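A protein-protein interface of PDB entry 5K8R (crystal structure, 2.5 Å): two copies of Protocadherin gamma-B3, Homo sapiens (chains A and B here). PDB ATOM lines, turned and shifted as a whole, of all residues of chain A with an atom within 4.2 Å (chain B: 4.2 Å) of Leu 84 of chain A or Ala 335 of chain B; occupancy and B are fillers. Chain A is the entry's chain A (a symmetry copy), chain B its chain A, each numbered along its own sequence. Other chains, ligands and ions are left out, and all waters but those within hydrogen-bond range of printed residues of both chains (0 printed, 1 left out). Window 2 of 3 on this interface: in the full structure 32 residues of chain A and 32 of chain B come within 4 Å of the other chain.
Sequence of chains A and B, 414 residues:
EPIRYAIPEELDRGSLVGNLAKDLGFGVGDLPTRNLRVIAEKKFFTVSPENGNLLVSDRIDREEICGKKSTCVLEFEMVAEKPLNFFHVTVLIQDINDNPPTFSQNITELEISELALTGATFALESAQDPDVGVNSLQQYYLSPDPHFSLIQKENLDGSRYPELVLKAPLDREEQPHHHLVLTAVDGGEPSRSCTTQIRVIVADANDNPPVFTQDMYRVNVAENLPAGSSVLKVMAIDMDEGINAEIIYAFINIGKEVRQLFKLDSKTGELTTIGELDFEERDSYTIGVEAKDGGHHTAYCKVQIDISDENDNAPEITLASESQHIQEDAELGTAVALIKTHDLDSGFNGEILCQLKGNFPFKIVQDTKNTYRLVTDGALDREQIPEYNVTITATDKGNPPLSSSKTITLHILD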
ATOM      1  N   ALA A  80     -35.545  14.598   2.428  1.00  0.00           N
ATOM      2  CA  ALA A  80     -35.568  13.150   2.518  1.00  0.00           C
ATOM      3  C   ALA A  80     -34.134  12.649   2.575  1.00  0.00           C
ATOM      4  O   ALA A  80     -33.205  13.322   2.120  1.00  0.00           O
ATOM      5  CB  ALA A  80     -36.297  12.517   1.327  1.00  0.00           C
ATOM      6  N   GLU A  81     -33.955  11.461   3.141  1.00  0.00           N
ATOM      7  CA  GLU A  81     -32.640  10.848   3.229  1.00  0.00           C
ATOM      8  C   GLU A  81     -32.684   9.456   2.613  1.00  0.00           C
ATOM      9  O   GLU A  81     -33.753   8.897   2.353  1.00  0.00           O
ATOM     10  CB  GLU A  81     -32.135  10.790   4.677  1.00  0.00           C
ATOM     11  CG  GLU A  81     -33.159  10.346   5.702  1.00  0.00           C
ATOM     12  CD  GLU A  81     -32.605  10.360   7.112  1.00  0.00           C
ATOM     13  OE1 GLU A  81     -31.470   9.877   7.310  1.00  0.00           O
ATOM     14  OE2 GLU A  81     -33.297  10.864   8.021  1.00  0.00           O
ATOM     15  N   LYS A  82     -31.493   8.909   2.380  1.00  0.00           N
ATOM     16  CA  LYS A  82     -31.318   7.633   1.689  1.00  0.00           C
ATOM     17  C   LYS A  82     -32.070   7.568   0.358  1.00  0.00           C
ATOM     18  O   LYS A  82     -33.030   6.808   0.227  1.00  0.00           O
ATOM     19  CB  LYS A  82     -31.758   6.477   2.591  1.00  0.00           C
ATOM     20  CG  LYS A  82     -30.949   6.351   3.869  1.00  0.00           C
ATOM     21  CD  LYS A  82     -31.429   5.186   4.715  1.00  0.00           C
ATOM     22  CE  LYS A  82     -30.592   5.037   5.973  1.00  0.00           C
ATOM     23  NZ  LYS A  82     -30.620   6.270   6.807  1.00  0.00           N
ATOM     24  N   PRO A  83     -31.641   8.365  -0.637  1.00  0.00           N
ATOM     25  CA  PRO A  83     -30.571   9.367  -0.573  1.00  0.00           C
ATOM     26  C   PRO A  83     -31.080  10.734  -0.117  1.00  0.00           C
ATOM     27  O   PRO A  83     -32.287  10.976  -0.139  1.00  0.00           O
ATOM     28  CB  PRO A  83     -30.071   9.424  -2.014  1.00  0.00           C
ATOM     29  CG  PRO A  83     -31.290   9.153  -2.819  1.00  0.00           C
ATOM     30  CD  PRO A  83     -32.125   8.179  -2.017  1.00  0.00           C
ATOM     31  N   LEU A  84     -30.168  11.611   0.296  1.00  0.00           N
ATOM     32  CA  LEU A  84     -30.551  12.949   0.727  1.00  0.00           C
ATOM     33  C   LEU A  84     -31.002  13.783  -0.465  1.00  0.00           C
ATOM     34  O   LEU A  84     -30.338  13.806  -1.506  1.00  0.00           O
ATOM     35  CB  LEU A  84     -29.385  13.634   1.437  1.00  0.00           C
ATOM     36  CG  LEU A  84     -29.178  13.300   2.915  1.00  0.00           C
ATOM     37  CD1 LEU A  84     -27.869  13.883   3.407  1.00  0.00           C
ATOM     38  CD2 LEU A  84     -30.339  13.827   3.742  1.00  0.00           C
ATOM     39  N   ASN A  85     -32.130  14.473  -0.309  1.00  0.00           N
ATOM     40  CA  ASN A  85     -32.685  15.290  -1.378  1.00  0.00           C
ATOM     41  C   ASN A  85     -33.623  16.334  -0.788  1.00  0.00           C
ATOM     42  O   ASN A  85     -34.325  16.069   0.193  1.00  0.00           O
ATOM     43  CB  ASN A  85     -33.436  14.435  -2.408  1.00  0.00           C
ATOM     44  CG  ASN A  85     -32.542  13.966  -3.540  1.00  0.00           C
ATOM     45  OD1 ASN A  85     -31.646  14.687  -3.980  1.00  0.00           O
ATOM     46  ND2 ASN A  85     -32.782  12.749  -4.018  1.00  0.00           N
ATOM     47  N   SER B 321     -28.820  16.315   7.108  1.00  0.00           N
ATOM     48  CA  SER B 321     -27.937  15.165   6.944  1.00  0.00           C
ATOM     49  C   SER B 321     -28.648  13.926   7.470  1.00  0.00           C
ATOM     50  O   SER B 321     -29.714  14.010   8.085  1.00  0.00           O
ATOM     51  CB  SER B 321     -26.601  15.369   7.666  1.00  0.00           C
ATOM     52  OG  SER B 321     -26.799  15.622   9.045  1.00  0.00           O
ATOM     53  N   GLU B 322     -28.038  12.767   7.215  1.00  0.00           N
ATOM     54  CA  GLU B 322     -28.547  11.490   7.721  1.00  0.00           C
ATOM     55  C   GLU B 322     -28.013  11.263   9.135  1.00  0.00           C
ATOM     56  O   GLU B 322     -27.121  10.448   9.381  1.00  0.00           O
ATOM     57  CB  GLU B 322     -28.158  10.350   6.790  1.00  0.00           C
ATOM     58  CG  GLU B 322     -28.673  10.483   5.372  1.00  0.00           C
ATOM     59  CD  GLU B 322     -28.498   9.207   4.571  1.00  0.00           C
ATOM     60  OE1 GLU B 322     -28.018   8.205   5.144  1.00  0.00           O
ATOM     61  OE2 GLU B 322     -28.839   9.206   3.369  1.00  0.00           O
ATOM     62  N   GLY B 333     -19.248  10.782  -4.650  1.00  0.00           N
ATOM     63  CA  GLY B 333     -20.424  11.482  -5.117  1.00  0.00           C
ATOM     64  C   GLY B 333     -21.656  11.309  -4.259  1.00  0.00           C
ATOM     65  O   GLY B 333     -22.717  11.834  -4.619  1.00  0.00           O
ATOM     66  N   THR B 334     -21.553  10.598  -3.141  1.00  0.00           N
ATOM     67  CA  THR B 334     -22.715  10.342  -2.300  1.00  0.00           C
ATOM     68  C   THR B 334     -23.147  11.613  -1.579  1.00  0.00           C
ATOM     69  O   THR B 334     -22.315  12.340  -1.026  1.00  0.00           O
ATOM     70  CB  THR B 334     -22.399   9.242  -1.286  1.00  0.00           C
ATOM     71  OG1 THR B 334     -22.012   8.049  -1.978  1.00  0.00           O
ATOM     72  CG2 THR B 334     -23.612   8.947  -0.415  1.00  0.00           C
ATOM     73  N   ALA B 335     -24.452  11.882  -1.589  1.00  0.00           N
ATOM     74  CA  ALA B 335     -24.992  13.005  -0.836  1.00  0.00           C
ATOM     75  C   ALA B 335     -24.772  12.789   0.655  1.00  0.00           C
ATOM     76  O   ALA B 335     -25.093  11.728   1.196  1.00  0.00           O
ATOM     77  CB  ALA B 335     -26.480  13.178  -1.136  1.00  0.00           C
ATOM     78  N   VAL B 336     -24.221  13.803   1.317  1.00  0.00           N
ATOM     79  CA  VAL B 336     -23.814  13.687   2.712  1.00  0.00           C
ATOM     80  C   VAL B 336     -24.518  14.752   3.544  1.00  0.00           C
ATOM     81  O   VAL B 336     -24.886  14.513   4.701  1.00  0.00           O
ATOM     82  CB  VAL B 336     -22.281  13.786   2.835  1.00  0.00           C
ATOM     83  CG1 VAL B 336     -21.845  13.791   4.287  1.00  0.00           C
ATOM     84  CG2 VAL B 336     -21.626  12.640   2.084  1.00  0.00           C
ATOM     85  N   ALA B 337     -24.727  15.929   2.958  1.00  0.00           N
ATOM     86  CA  ALA B 337     -25.422  17.005   3.645  1.00  0.00           C
ATOM     87  C   ALA B 337     -26.166  17.854   2.627  1.00  0.00           C
ATOM     88  O   ALA B 337     -25.784  17.927   1.456  1.00  0.00           O
ATOM     89  CB  ALA B 337     -24.454  17.874   4.458  1.00  0.00           C
ATOM     90  N   LEU B 338     -27.239  18.491   3.088  1.00  0.00           N
ATOM     91  CA  LEU B 338     -28.048  19.387   2.275  1.00  0.00           C
ATOM     92  C   LEU B 338     -27.898  20.806   2.801  1.00  0.00           C
ATOM     93  O   LEU B 338     -27.982  21.036   4.014  1.00  0.00           O
ATOM     94  CB  LEU B 338     -29.519  18.965   2.290  1.00  0.00           C
ATOM     95  CG  LEU B 338     -29.835  17.558   1.778  1.00  0.00           C
ATOM     96  CD1 LEU B 338     -31.333  17.292   1.825  1.00  0.00           C
ATOM     97  CD2 LEU B 338     -29.297  17.364   0.370  1.00  0.00           C
ATOM     98  N   LEU B 374     -23.563  18.760  -0.162  1.00  0.00           N
ATOM     99  CA  LEU B 374     -22.215  18.379   0.238  1.00  0.00           C
ATOM    100  C   LEU B 374     -21.986  16.927  -0.162  1.00  0.00           C
ATOM    101  O   LEU B 374     -22.666  16.025   0.336  1.00  0.00           O
ATOM    102  CB  LEU B 374     -22.027  18.570   1.741  1.00  0.00           C
ATOM    103  CG  LEU B 374     -20.601  18.420   2.269  1.00  0.00           C
ATOM    104  CD1 LEU B 374     -19.700  19.497   1.683  1.00  0.00           C
ATOM    105  CD2 LEU B 374     -20.585  18.468   3.788  1.00  0.00           C
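The side-chain carboxylate (OE1) of Glu 322 of chain B lies within salt-bridge range of the side-chain amino group (NZ) of Lys 82 of chain A, at 3.6 Å.
N of Val 336 of chain B sits at hydrogen-bond distance from O of Leu 374 of chain B, 2.9 Å away.
The backbone NH of Leu 374 of chain B lies within hydrogen-bond range of the backbone carbonyl oxygen of Ala 337 of chain B, at 2.9 Å.
The backbone carbonyl oxygen (O) of Ala 80 of chain A sits at hydrogen-bond distance from the backbone NH (N) of Asn 85 of chain A (2.9 Å).
OE1 of Glu 81 of chain A is in salt-bridge range of NZ of Lys 82 of chain A, at 3.7 Å.
Among the printed residues, pairs that only touch across the chains: Leu 84 of chain A with Val 336 of chain B, Glu 81 of chain A with Glu 322 of chain B, Asn 85 of chain A with Leu 338 of chain B, Leu 84 of chain A with Ser 321 of chain B, Leu 84 of chain A with Glu 322 of chain B, Leu 84 of chain A with Ala 337 of chain B, Leu 84 of chain A with Leu 338 of chain B and Leu 84 of chain A with Ala 335 of chain B.
Of chain B, only Ser 321 (3.8 Å), Glu 322 (3.8 Å), Ala 335 (3.9 Å), Val 336 (3.3 Å), Ala 337 (3.8 Å) and Leu 338 (3.9 Å) come within 4 Å of Leu 84 of chain A.
Of the printed residues of chain A, Ala 335 of chain B touches Leu 84.
Printed residues of chain A within 4 Å of Ala 337 of chain B: Leu 84 (3.8 Å).
Of the printed residues of chain B, Lys 82 of chain A touches Glu 322 (2.8 Å).
The nearest printed residue of chain B that does not touch Leu 84 of chain A is Leu 374 of chain B (6.4 Å).
The nearest printed residue of chain B that does not touch Glu 81 of chain A is Ser 321 of chain B (4.6 Å).
Of the 6 printed residues of chain A, 4 touch a printed residue of chain B.
Hydrophobic or aromatic side chains of chain A within 4 Å of the printed part of chain B: Leu 84.
Of the 9 printed residues of chain B, 6 touch a printed residue of chain A.
Hydrophobic or aromatic side chains of chain B that line the printed part of chain A: Ala 335 and Leu 338.
Along chain B the printed residues that touch a printed residue of chain A span positions 321 to 338.
Among the printed residues, 9 pairs touch across the chains.
Among the printed residues, Asp or Glu carboxylates within 4 Å of a Lys or Arg side-chain nitrogen of the other chain: Lys 82 of chain A with Glu 322 of chain B (3.6 Å).
No position is printed for both chains.
Of the 9 pairs that touch across the chains among the printed residues, none has its exchanged pair printed and touching as well.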
